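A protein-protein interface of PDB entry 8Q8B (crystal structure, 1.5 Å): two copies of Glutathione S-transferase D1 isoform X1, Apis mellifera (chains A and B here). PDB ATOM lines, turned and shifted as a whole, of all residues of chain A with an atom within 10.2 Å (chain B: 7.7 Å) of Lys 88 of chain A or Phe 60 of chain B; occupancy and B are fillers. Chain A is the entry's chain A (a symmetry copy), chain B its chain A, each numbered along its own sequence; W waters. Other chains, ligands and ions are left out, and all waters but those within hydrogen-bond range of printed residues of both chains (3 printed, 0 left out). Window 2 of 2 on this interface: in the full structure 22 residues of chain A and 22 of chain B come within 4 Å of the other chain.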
ATOM      1  N   TYR A  83      16.977  17.107  15.178  1.00  0.00           N
ATOM      2  CA  TYR A  83      15.555  16.842  15.381  1.00  0.00           C
ATOM      3  C   TYR A  83      15.400  15.333  15.300  1.00  0.00           C
ATOM      4  O   TYR A  83      15.107  14.770  14.237  1.00  0.00           O
ATOM      5  CB  TYR A  83      14.698  17.588  14.350  1.00  0.00           C
ATOM      6  CG  TYR A  83      13.215  17.628  14.656  1.00  0.00           C
ATOM      7  CD1 TYR A  83      12.740  17.968  15.920  1.00  0.00           C
ATOM      8  CD2 TYR A  83      12.282  17.353  13.655  1.00  0.00           C
ATOM      9  CE1 TYR A  83      11.367  18.014  16.182  1.00  0.00           C
ATOM     10  CE2 TYR A  83      10.930  17.399  13.907  1.00  0.00           C
ATOM     11  CZ  TYR A  83      10.467  17.742  15.150  1.00  0.00           C
ATOM     12  OH  TYR A  83       9.098  17.778  15.386  1.00  0.00           O
ATOM     13  N   PRO A  84      15.700  14.632  16.393  1.00  0.00           N
ATOM     14  CA  PRO A  84      15.822  13.177  16.324  1.00  0.00           C
ATOM     15  C   PRO A  84      14.543  12.515  15.843  1.00  0.00           C
ATOM     16  O   PRO A  84      13.436  12.929  16.187  1.00  0.00           O
ATOM     17  CB  PRO A  84      16.146  12.785  17.771  1.00  0.00           C
ATOM     18  CG  PRO A  84      16.784  13.972  18.352  1.00  0.00           C
ATOM     19  CD  PRO A  84      16.090  15.152  17.715  1.00  0.00           C
ATOM     20  N   LYS A  85      14.714  11.465  15.040  1.00  0.00           N
ATOM     21  CA  LYS A  85      13.575  10.664  14.615  1.00  0.00           C
ATOM     22  C   LYS A  85      12.962   9.906  15.781  1.00  0.00           C
ATOM     23  O   LYS A  85      11.757   9.636  15.783  1.00  0.00           O
ATOM     24  CB  LYS A  85      14.005   9.697  13.509  1.00  0.00           C
ATOM     25  CG  LYS A  85      14.433  10.403  12.236  1.00  0.00           C
ATOM     26  CD  LYS A  85      14.864   9.419  11.160  1.00  0.00           C
ATOM     27  CE  LYS A  85      15.249  10.144   9.876  1.00  0.00           C
ATOM     28  NZ  LYS A  85      14.702   9.454   8.667  1.00  0.00           N
ATOM     29  N   ASP A  86      13.768   9.551  16.782  1.00  0.00           N
ATOM     30  CA  ASP A  86      13.245   8.854  17.940  1.00  0.00           C
ATOM     31  C   ASP A  86      12.084   9.630  18.545  1.00  0.00           C
ATOM     32  O   ASP A  86      12.191  10.833  18.789  1.00  0.00           O
ATOM     33  CB  ASP A  86      14.352   8.677  18.974  1.00  0.00           C
ATOM     34  CG  ASP A  86      13.837   8.081  20.252  1.00  0.00           C
ATOM     35  OD1 ASP A  86      13.621   6.852  20.291  1.00  0.00           O
ATOM     36  OD2 ASP A  86      13.587   8.838  21.206  1.00  0.00           O
ATOM     37  N   LEU A  87      10.968   8.938  18.777  1.00  0.00           N
ATOM     38  CA  LEU A  87       9.735   9.655  19.079  1.00  0.00           C
ATOM     39  C   LEU A  87       9.754  10.297  20.460  1.00  0.00           C
ATOM     40  O   LEU A  87       9.219  11.394  20.629  1.00  0.00           O
ATOM     41  CB  LEU A  87       8.528   8.742  18.929  1.00  0.00           C
ATOM     42  CG  LEU A  87       8.305   8.324  17.473  1.00  0.00           C
ATOM     43  CD1 LEU A  87       7.128   7.400  17.389  1.00  0.00           C
ATOM     44  CD2 LEU A  87       8.114   9.557  16.574  1.00  0.00           C
ATOM     45  N   LYS A  88      10.351   9.645  21.470  1.00  0.00           N
ATOM     46  CA  LYS A  88      10.450  10.292  22.778  1.00  0.00           C
ATOM     47  C   LYS A  88      11.363  11.508  22.733  1.00  0.00           C
ATOM     48  O   LYS A  88      11.024  12.569  23.272  1.00  0.00           O
ATOM     49  CB  LYS A  88      10.950   9.290  23.824  1.00  0.00           C
ATOM     50  CG  LYS A  88       9.915   8.256  24.210  1.00  0.00           C
ATOM     51  CD  LYS A  88      10.397   7.403  25.405  1.00  0.00           C
ATOM     52  CE  LYS A  88      11.434   6.387  24.981  1.00  0.00           C
ATOM     53  NZ  LYS A  88      10.844   5.344  24.100  1.00  0.00           N
ATOM     54  N   LYS A  89      12.515  11.390  22.077  1.00  0.00           N
ATOM     55  CA  LYS A  89      13.409  12.533  21.979  1.00  0.00           C
ATOM     56  C   LYS A  89      12.762  13.653  21.180  1.00  0.00           C
ATOM     57  O   LYS A  89      12.864  14.828  21.544  1.00  0.00           O
ATOM     58  CB  LYS A  89      14.734  12.093  21.368  1.00  0.00           C
ATOM     59  CG  LYS A  89      15.550  11.216  22.348  1.00  0.00           C
ATOM     60  CD  LYS A  89      16.768  10.655  21.656  1.00  0.00           C
ATOM     61  CE  LYS A  89      17.513   9.680  22.565  1.00  0.00           C
ATOM     62  NZ  LYS A  89      18.701   9.122  21.851  1.00  0.00           N
ATOM     63  N   ARG A  90      12.094  13.303  20.084  1.00  0.00           N
ATOM     64  CA  ARG A  90      11.416  14.312  19.285  1.00  0.00           C
ATOM     65  C   ARG A  90      10.325  15.006  20.090  1.00  0.00           C
ATOM     66  O   ARG A  90      10.138  16.229  19.982  1.00  0.00           O
ATOM     67  CB  ARG A  90      10.839  13.646  18.044  1.00  0.00           C
ATOM     68  CG  ARG A  90      10.078  14.621  17.166  1.00  0.00           C
ATOM     69  CD  ARG A  90       9.804  14.039  15.783  1.00  0.00           C
ATOM     70  NE  ARG A  90      11.049  13.888  15.052  1.00  0.00           N
ATOM     71  CZ  ARG A  90      11.180  14.042  13.745  1.00  0.00           C
ATOM     72  NH1 ARG A  90      10.143  14.351  12.970  1.00  0.00           N
ATOM     73  NH2 ARG A  90      12.385  13.905  13.204  1.00  0.00           N
ATOM     74  N   ALA A  91       9.587  14.241  20.894  1.00  0.00           N
ATOM     75  CA  ALA A  91       8.531  14.829  21.709  1.00  0.00           C
ATOM     76  C   ALA A  91       9.083  15.879  22.659  1.00  0.00           C
ATOM     77  O   ALA A  91       8.447  16.916  22.876  1.00  0.00           O
ATOM     78  CB  ALA A  91       7.788  13.743  22.485  1.00  0.00           C
ATOM     79  N   ILE A  92      10.265  15.637  23.237  1.00  0.00           N
ATOM     80  CA  ILE A  92      10.835  16.625  24.153  1.00  0.00           C
ATOM     81  C   ILE A  92      11.280  17.877  23.398  1.00  0.00           C
ATOM     82  O   ILE A  92      11.102  19.001  23.887  1.00  0.00           O
ATOM     83  CB  ILE A  92      11.988  16.010  24.970  1.00  0.00           C
ATOM     84  CG1 ILE A  92      11.463  14.854  25.823  1.00  0.00           C
ATOM     85  CG2 ILE A  92      12.638  17.077  25.855  1.00  0.00           C
ATOM     86  CD1 ILE A  92      10.361  15.270  26.796  1.00  0.00           C
ATOM     87  N   VAL A  93      11.838  17.724  22.187  1.00  0.00           N
ATOM     88  CA  VAL A  93      12.133  18.906  21.378  1.00  0.00           C
ATOM     89  C   VAL A  93      10.849  19.677  21.094  1.00  0.00           C
ATOM     90  O   VAL A  93      10.796  20.899  21.246  1.00  0.00           O
ATOM     91  CB  VAL A  93      12.856  18.526  20.076  1.00  0.00           C
ATOM     92  CG1 VAL A  93      13.107  19.783  19.247  1.00  0.00           C
ATOM     93  CG2 VAL A  93      14.183  17.796  20.382  1.00  0.00           C
ATOM     94  N   ASN A  94       9.786  18.968  20.709  1.00  0.00           N
ATOM     95  CA  ASN A  94       8.525  19.649  20.428  1.00  0.00           C
ATOM     96  C   ASN A  94       8.010  20.360  21.664  1.00  0.00           C
ATOM     97  O   ASN A  94       7.592  21.522  21.603  1.00  0.00           O
ATOM     98  CB  ASN A  94       7.485  18.654  19.937  1.00  0.00           C
ATOM     99  CG  ASN A  94       7.806  18.107  18.565  1.00  0.00           C
ATOM    100  OD1 ASN A  94       8.532  18.727  17.795  1.00  0.00           O
ATOM    101  ND2 ASN A  94       7.245  16.946  18.246  1.00  0.00           N
ATOM    102  N   GLN A  95       8.043  19.672  22.801  1.00  0.00           N
ATOM    103  CA  GLN A  95       7.621  20.283  24.052  1.00  0.00           C
ATOM    104  C   GLN A  95       8.393  21.571  24.315  1.00  0.00           C
ATOM    105  O   GLN A  95       7.809  22.609  24.653  1.00  0.00           O
ATOM    106  CB  GLN A  95       7.834  19.286  25.178  1.00  0.00           C
ATOM    107  CG  GLN A  95       7.592  19.809  26.550  1.00  0.00           C
ATOM    108  CD  GLN A  95       8.144  18.830  27.579  1.00  0.00           C
ATOM    109  OE1 GLN A  95       9.304  18.923  27.992  1.00  0.00           O
ATOM    110  NE2 GLN A  95       7.334  17.857  27.949  1.00  0.00           N
ATOM    111  N   ARG A  96       9.709  21.529  24.149  1.00  0.00           N
ATOM    112  CA  ARG A  96      10.497  22.722  24.438  1.00  0.00           C
ATOM    113  C   ARG A  96      10.226  23.837  23.435  1.00  0.00           C
ATOM    114  O   ARG A  96      10.310  25.015  23.788  1.00  0.00           O
ATOM    115  CB  ARG A  96      11.983  22.384  24.466  1.00  0.00           C
ATOM    116  CG  ARG A  96      12.832  23.406  25.198  1.00  0.00           C
ATOM    117  CD  ARG A  96      12.659  23.322  26.726  1.00  0.00           C
ATOM    118  NE  ARG A  96      13.140  22.059  27.279  1.00  0.00           N
ATOM    119  CZ  ARG A  96      12.362  21.058  27.663  1.00  0.00           C
ATOM    120  NH1 ARG A  96      11.041  21.158  27.639  1.00  0.00           N
ATOM    121  NH2 ARG A  96      12.920  19.928  28.089  1.00  0.00           N
ATOM    122  N   ALA A 148      17.026  20.398  25.346  1.00  0.00           N
ATOM    123  CA  ALA A 148      15.990  19.422  25.048  1.00  0.00           C
ATOM    124  C   ALA A 148      16.605  18.137  24.507  1.00  0.00           C
ATOM    125  O   ALA A 148      16.209  17.620  23.463  1.00  0.00           O
ATOM    126  CB  ALA A 148      14.969  20.012  24.073  1.00  0.00           C
ATOM    127  N   GLY A 149      17.581  17.595  25.226  1.00  0.00           N
ATOM    128  CA  GLY A 149      18.203  16.356  24.819  1.00  0.00           C
ATOM    129  C   GLY A 149      19.696  16.348  25.060  1.00  0.00           C
ATOM    130  O   GLY A 149      20.260  17.330  25.555  1.00  0.00           O
ATOM    131  N   LYS A 150      20.344  15.249  24.678  1.00  0.00           N
ATOM    132  CA  LYS A 150      21.774  15.085  24.885  1.00  0.00           C
ATOM    133  C   LYS A 150      22.615  15.758  23.812  1.00  0.00           C
ATOM    134  O   LYS A 150      23.838  15.811  23.957  1.00  0.00           O
ATOM    135  CB  LYS A 150      22.124  13.595  24.954  1.00  0.00           C
ATOM    136  CG  LYS A 150      21.386  12.817  26.030  1.00  0.00           C
ATOM    137  CD  LYS A 150      21.581  11.325  25.816  1.00  0.00           C
ATOM    138  CE  LYS A 150      20.857  10.501  26.870  1.00  0.00           C
ATOM    139  NZ  LYS A 150      21.019   9.038  26.633  1.00  0.00           N
ATOM    140  N   THR A 153      19.723  20.674  19.585  1.00  0.00           N
ATOM    141  CA  THR A 153      18.533  20.443  18.773  1.00  0.00           C
ATOM    142  C   THR A 153      17.963  21.773  18.314  1.00  0.00           C
ATOM    143  O   THR A 153      18.439  22.852  18.681  1.00  0.00           O
ATOM    144  CB  THR A 153      17.425  19.694  19.520  1.00  0.00           C
ATOM    145  OG1 THR A 153      16.936  20.513  20.587  1.00  0.00           O
ATOM    146  CG2 THR A 153      17.899  18.336  20.066  1.00  0.00           C
ATOM    147  N   MET B   1      -0.389   3.132  29.885  1.00  0.00           N
ATOM    148  CA  MET B   1      -0.213   4.574  29.838  1.00  0.00           C
ATOM    149  C   MET B   1      -1.122   5.281  30.839  1.00  0.00           C
ATOM    150  O   MET B   1      -2.334   5.101  30.806  1.00  0.00           O
ATOM    151  CB  MET B   1      -0.499   5.078  28.428  1.00  0.00           C
ATOM    152  CG  MET B   1      -0.271   6.538  28.268  1.00  0.00           C
ATOM    153  SD  MET B   1      -0.600   7.091  26.589  1.00  0.00           S
ATOM    154  CE  MET B   1       0.383   5.961  25.623  1.00  0.00           C
ATOM    155  N   ASP B   2      -0.543   6.100  31.712  1.00  0.00           N
ATOM    156  CA  ASP B   2      -1.335   6.901  32.636  1.00  0.00           C
ATOM    157  C   ASP B   2      -1.560   8.282  32.042  1.00  0.00           C
ATOM    158  O   ASP B   2      -0.666   8.844  31.411  1.00  0.00           O
ATOM    159  CB  ASP B   2      -0.643   7.032  33.993  1.00  0.00           C
ATOM    160  CG  ASP B   2      -0.501   5.706  34.709  1.00  0.00           C
ATOM    161  OD1 ASP B   2      -1.276   4.775  34.401  1.00  0.00           O
ATOM    162  OD2 ASP B   2       0.378   5.615  35.594  1.00  0.00           O
ATOM    163  N   THR B  54      -0.658  15.501  31.481  1.00  0.00           N
ATOM    164  CA  THR B  54       0.613  14.803  31.451  1.00  0.00           C
ATOM    165  C   THR B  54       0.311  13.332  31.221  1.00  0.00           C
ATOM    166  O   THR B  54      -0.636  12.797  31.807  1.00  0.00           O
ATOM    167  CB  THR B  54       1.396  14.983  32.775  1.00  0.00           C
ATOM    168  OG1 THR B  54       1.859  16.337  32.877  1.00  0.00           O
ATOM    169  CG2 THR B  54       2.587  14.049  32.818  1.00  0.00           C
ATOM    170  N   ILE B  55       1.096  12.682  30.371  1.00  0.00           N
ATOM    171  CA  ILE B  55       1.037  11.232  30.260  1.00  0.00           C
ATOM    172  C   ILE B  55       2.298  10.648  30.869  1.00  0.00           C
ATOM    173  O   ILE B  55       3.352  11.287  30.943  1.00  0.00           O
ATOM    174  CB  ILE B  55       0.858  10.718  28.811  1.00  0.00           C
ATOM    175  CG1 ILE B  55       2.027  11.149  27.928  1.00  0.00           C
ATOM    176  CG2 ILE B  55      -0.487  11.129  28.263  1.00  0.00           C
ATOM    177  CD1 ILE B  55       2.102  10.418  26.586  1.00  0.00           C
ATOM    178  N   ASP B  56       2.166   9.409  31.322  1.00  0.00           N
ATOM    179  CA  ASP B  56       3.285   8.585  31.751  1.00  0.00           C
ATOM    180  C   ASP B  56       3.142   7.309  30.943  1.00  0.00           C
ATOM    181  O   ASP B  56       2.200   6.540  31.168  1.00  0.00           O
ATOM    182  CB  ASP B  56       3.229   8.324  33.260  1.00  0.00           C
ATOM    183  CG  ASP B  56       4.442   7.575  33.779  1.00  0.00           C
ATOM    184  OD1 ASP B  56       5.016   6.765  33.039  1.00  0.00           O
ATOM    185  OD2 ASP B  56       4.808   7.791  34.953  1.00  0.00           O
ATOM    186  N   ASP B  57       4.013   7.139  29.951  1.00  0.00           N
ATOM    187  CA  ASP B  57       3.984   6.008  29.030  1.00  0.00           C
ATOM    188  C   ASP B  57       5.163   5.120  29.401  1.00  0.00           C
ATOM    189  O   ASP B  57       6.286   5.332  28.941  1.00  0.00           O
ATOM    190  CB  ASP B  57       4.058   6.494  27.579  1.00  0.00           C
ATOM    191  CG  ASP B  57       3.901   5.368  26.578  1.00  0.00           C
ATOM    192  OD1 ASP B  57       3.742   4.198  26.996  1.00  0.00           O
ATOM    193  OD2 ASP B  57       3.925   5.637  25.367  1.00  0.00           O
ATOM    194  N   ASN B  58       4.902   4.143  30.287  1.00  0.00           N
ATOM    195  CA  ASN B  58       5.914   3.178  30.725  1.00  0.00           C
ATOM    196  C   ASN B  58       7.159   3.897  31.239  1.00  0.00           C
ATOM    197  O   ASN B  58       8.294   3.547  30.907  1.00  0.00           O
ATOM    198  CB  ASN B  58       6.257   2.210  29.588  1.00  0.00           C
ATOM    199  CG  ASN B  58       7.115   1.046  30.050  1.00  0.00           C
ATOM    200  OD1 ASN B  58       7.053   0.649  31.202  1.00  0.00           O
ATOM    201  ND2 ASN B  58       7.934   0.513  29.151  1.00  0.00           N
ATOM    202  N   GLY B  59       6.941   4.958  32.011  1.00  0.00           N
ATOM    203  CA  GLY B  59       8.014   5.721  32.597  1.00  0.00           C
ATOM    204  C   GLY B  59       8.379   6.982  31.850  1.00  0.00           C
ATOM    205  O   GLY B  59       9.066   7.843  32.414  1.00  0.00           O
ATOM    206  N   PHE B  60       7.960   7.105  30.595  1.00  0.00           N
ATOM    207  CA  PHE B  60       8.244   8.299  29.812  1.00  0.00           C
ATOM    208  C   PHE B  60       7.198   9.346  30.149  1.00  0.00           C
ATOM    209  O   PHE B  60       6.006   9.163  29.877  1.00  0.00           O
ATOM    210  CB  PHE B  60       8.256   7.976  28.323  1.00  0.00           C
ATOM    211  CG  PHE B  60       8.289   9.193  27.451  1.00  0.00           C
ATOM    212  CD1 PHE B  60       9.337  10.090  27.540  1.00  0.00           C
ATOM    213  CD2 PHE B  60       7.286   9.424  26.524  1.00  0.00           C
ATOM    214  CE1 PHE B  60       9.368  11.220  26.724  1.00  0.00           C
ATOM    215  CE2 PHE B  60       7.314  10.545  25.712  1.00  0.00           C
ATOM    216  CZ  PHE B  60       8.354  11.437  25.812  1.00  0.00           C
ATOM    217  N   ARG B  61       7.637  10.420  30.794  1.00  0.00           N
ATOM    218  CA  ARG B  61       6.737  11.473  31.226  1.00  0.00           C
ATOM    219  C   ARG B  61       6.689  12.554  30.164  1.00  0.00           C
ATOM    220  O   ARG B  61       7.732  13.010  29.692  1.00  0.00           O
ATOM    221  CB  ARG B  61       7.209  12.057  32.554  1.00  0.00           C
ATOM    222  CG  ARG B  61       6.930  11.153  33.736  1.00  0.00           C
ATOM    223  CD  ARG B  61       5.638  11.593  34.384  1.00  0.00           C
ATOM    224  NE  ARG B  61       5.151  10.678  35.402  1.00  0.00           N
ATOM    225  CZ  ARG B  61       4.436  11.057  36.451  1.00  0.00           C
ATOM    226  NH1 ARG B  61       4.165  12.334  36.677  1.00  0.00           N
ATOM    227  NH2 ARG B  61       3.995  10.135  37.301  1.00  0.00           N
ATOM    228  N   LEU B  62       5.483  12.964  29.788  1.00  0.00           N
ATOM    229  CA  LEU B  62       5.339  13.980  28.748  1.00  0.00           C
ATOM    230  C   LEU B  62       4.184  14.904  29.088  1.00  0.00           C
ATOM    231  O   LEU B  62       3.040  14.462  29.209  1.00  0.00           O
ATOM    232  CB  LEU B  62       5.132  13.333  27.377  1.00  0.00           C
ATOM    233  CG  LEU B  62       5.142  14.301  26.198  1.00  0.00           C
ATOM    234  CD1 LEU B  62       6.492  14.972  26.064  1.00  0.00           C
ATOM    235  CD2 LEU B  62       4.820  13.540  24.934  1.00  0.00           C
ATOM    236  N   TRP B  63       4.501  16.181  29.273  1.00  0.00           N
ATOM    237  CA  TRP B  63       3.528  17.259  29.348  1.00  0.00           C
ATOM    238  C   TRP B  63       3.579  18.068  28.056  1.00  0.00           C
ATOM    239  O   TRP B  63       4.460  17.870  27.217  1.00  0.00           O
ATOM    240  CB  TRP B  63       3.796  18.151  30.572  1.00  0.00           C
ATOM    241  CG  TRP B  63       5.206  18.701  30.643  1.00  0.00           C
ATOM    242  CD1 TRP B  63       6.294  18.096  31.219  1.00  0.00           C
ATOM    243  CD2 TRP B  63       5.672  19.971  30.157  1.00  0.00           C
ATOM    244  NE1 TRP B  63       7.403  18.899  31.103  1.00  0.00           N
ATOM    245  CE2 TRP B  63       7.052  20.054  30.449  1.00  0.00           C
ATOM    246  CE3 TRP B  63       5.061  21.040  29.489  1.00  0.00           C
ATOM    247  CZ2 TRP B  63       7.827  21.169  30.111  1.00  0.00           C
ATOM    248  CZ3 TRP B  63       5.835  22.150  29.143  1.00  0.00           C
ATOM    249  CH2 TRP B  63       7.205  22.205  29.451  1.00  0.00           C
ATOM    250  N   ALA B  67       2.363  18.404  22.185  1.00  0.00           N
ATOM    251  CA  ALA B  67       3.480  17.468  22.050  1.00  0.00           C
ATOM    252  C   ALA B  67       3.037  16.045  22.366  1.00  0.00           C
ATOM    253  O   ALA B  67       3.516  15.092  21.738  1.00  0.00           O
ATOM    254  CB  ALA B  67       4.641  17.860  22.974  1.00  0.00           C
ATOM    255  N   ILE B  68       2.120  15.889  23.328  1.00  0.00           N
ATOM    256  CA  ILE B  68       1.550  14.573  23.604  1.00  0.00           C
ATOM    257  C   ILE B  68       0.806  14.063  22.380  1.00  0.00           C
ATOM    258  O   ILE B  68       0.956  12.905  21.972  1.00  0.00           O
ATOM    259  CB  ILE B  68       0.625  14.622  24.832  1.00  0.00           C
ATOM    260  CG1 ILE B  68       1.388  15.006  26.106  1.00  0.00           C
ATOM    261  CG2 ILE B  68      -0.055  13.287  24.979  1.00  0.00           C
ATOM    262  CD1 ILE B  68       0.462  15.318  27.264  1.00  0.00           C
ATOM    263  N   TYR B  71       3.117  12.904  19.659  1.00  0.00           N
ATOM    264  CA  TYR B  71       3.790  11.692  20.111  1.00  0.00           C
ATOM    265  C   TYR B  71       2.871  10.487  19.976  1.00  0.00           C
ATOM    266  O   TYR B  71       3.256   9.466  19.393  1.00  0.00           O
ATOM    267  CB  TYR B  71       4.263  11.858  21.557  1.00  0.00           C
ATOM    268  CG  TYR B  71       4.680  10.564  22.215  1.00  0.00           C
ATOM    269  CD1 TYR B  71       5.907   9.976  21.918  1.00  0.00           C
ATOM    270  CD2 TYR B  71       3.853   9.945  23.123  1.00  0.00           C
ATOM    271  CE1 TYR B  71       6.284   8.781  22.526  1.00  0.00           C
ATOM    272  CE2 TYR B  71       4.216   8.750  23.728  1.00  0.00           C
ATOM    273  CZ  TYR B  71       5.428   8.189  23.417  1.00  0.00           C
ATOM    274  OH  TYR B  71       5.787   7.004  24.029  1.00  0.00           O
ATOM    275  N   GLN B  75       3.602   7.312  17.591  1.00  0.00           N
ATOM    276  CA  GLN B  75       3.993   6.096  18.292  1.00  0.00           C
ATOM    277  C   GLN B  75       2.923   5.028  18.201  1.00  0.00           C
ATOM    278  O   GLN B  75       3.250   3.833  18.205  1.00  0.00           O
ATOM    279  CB  GLN B  75       4.312   6.409  19.755  1.00  0.00           C
ATOM    280  CG  GLN B  75       4.869   5.202  20.540  1.00  0.00           C
ATOM    281  CD  GLN B  75       6.245   4.797  20.059  1.00  0.00           C
ATOM    282  OE1 GLN B  75       7.256   5.328  20.519  1.00  0.00           O
ATOM    283  NE2 GLN B  75       6.295   3.865  19.106  1.00  0.00           N
ATOM    284  N   TYR B  76       1.652   5.422  18.105  1.00  0.00           N
ATOM    285  CA  TYR B  76       0.565   4.460  18.176  1.00  0.00           C
ATOM    286  C   TYR B  76      -0.429   4.518  17.027  1.00  0.00           C
ATOM    287  O   TYR B  76      -1.373   3.723  17.020  1.00  0.00           O
ATOM    288  CB  TYR B  76      -0.204   4.630  19.490  1.00  0.00           C
ATOM    289  CG  TYR B  76       0.652   4.407  20.700  1.00  0.00           C
ATOM    290  CD1 TYR B  76       0.939   3.115  21.134  1.00  0.00           C
ATOM    291  CD2 TYR B  76       1.170   5.471  21.418  1.00  0.00           C
ATOM    292  CE1 TYR B  76       1.727   2.899  22.237  1.00  0.00           C
ATOM    293  CE2 TYR B  76       1.958   5.257  22.533  1.00  0.00           C
ATOM    294  CZ  TYR B  76       2.234   3.968  22.933  1.00  0.00           C
ATOM    295  OH  TYR B  76       3.018   3.741  24.040  1.00  0.00           O
HETATM  296  O   HOH W   1       8.181  15.687  29.792  1.00  0.00           O
HETATM  297  O   HOH W   2       8.023   5.496  23.136  1.00  0.00           O
HETATM  298  O   HOH W   3       5.660  14.992  19.939  1.00  0.00           O
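The backbone carbonyl oxygen (O) of Trp 63 of chain B lies within hydrogen-bond range of the side-chain amide nitrogen (NE2) of Gln 95 of chain A, at 3.0 Å.
OE1 of Gln 95 of chain A sits at hydrogen-bond distance from NH1 of Arg 96 of chain A (2.9 Å).
The side-chain hydroxyl of Tyr 71 of chain B is in hydrogen-bond range of the side-chain carboxylate of Asp 57 of chain B (2.7 Å).
The side-chain carboxylate (OD2) of Asp 86 of chain A sits at hydrogen-bond distance from the backbone NH (N) of Lys 88 of chain A (3.3 Å).
O of Leu 62 of chain B sits at hydrogen-bond distance from N of Ile 55 of chain B, at 2.9 Å.
Tyr 71 of chain B touches Leu 87 of chain A.
Leu 87 of chain A touches Gln 75 of chain B.
Phe 60 of chain B touches Lys 88 of chain A.
Leu 62 of chain B touches Ala 91 of chain A.
Ala 91 of chain A touches Ala 67 of chain B.
Ile 92 of chain A touches Leu 62 of chain B.
Leu 62 of chain B touches Gln 95 of chain A (CD1 to NE2, 3.5 Å).
Ala 67 of chain B touches Gln 95 of chain A (CB to N, 3.9 Å).
Lys 88 of chain A touches just one residue of chain B: Phe 60.
Phe 60 of chain B touches just one residue of chain A: Lys 88 (3.4 Å).
No residue of chain A comes within 4 Å of Asp 56 of chain B.
No residue of chain A comes within 4 Å of Asp 57 of chain B.
No residue of chain A comes within 4 Å of Gly 59 of chain B.
Of the printed residues of chain A, Tyr 71 of chain B touches Leu 87.
Printed residues of chain B within 4 Å of Ala 91 of chain A: Leu 62 and Ala 67.
Of the printed residues of chain A, Trp 63 of chain B touches Gln 95 (3.0 Å).
Of the printed residues of chain B, Ile 92 of chain A touches Leu 62.
Of the printed residues of chain B, Leu 87 of chain A touches Tyr 71 and Gln 75.
Ile 68 of chain B touches none of the printed residues of chain A.
The nearest residue of chain B that does not touch Lys 88 of chain A is Tyr 71 of chain B (4.04 Å).
The nearest residue of chain A that does not touch Phe 60 of chain B is Ala 91 of chain A (4.1 Å).
Hydrophobic or aromatic side chains of chain A that line the printed part of chain B: Leu 87, Ala 91 and Ile 92.
Along chain A the printed residues that touch a printed residue of chain B span positions 87 to 95.
Among the printed residues, 9 pairs touch across the chains.
No position is printed for both chains.
Of the 9 pairs that touch across the chains among the printed residues, none has its exchanged pair printed and touching as well.
Water W1 lies within hydrogen-bond range of the backbone carbonyl oxygen (O) of Arg 61 of chain B (2.7 Å) and the side-chain amide nitrogen (NE2) of Gln 95 of chain A (3.0 Å).
Water W2 lies within hydrogen-bond range of the side-chain amide oxygen of Gln 75 of chain B (2.7 Å), the side-chain hydroxyl of Tyr 71 of chain B (2.8 Å) and the side-chain amino group of Lys 88 of chain A (3.0 Å).
Water W3 lies within hydrogen-bond range of the backbone carbonyl oxygen (O) of Ala 67 of chain B (2.8 Å), the side-chain amide nitrogen (ND2) of Asn 94 of chain A (3.0 Å) and the backbone NH (N) of Tyr 71 of chain B (3.3 Å).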
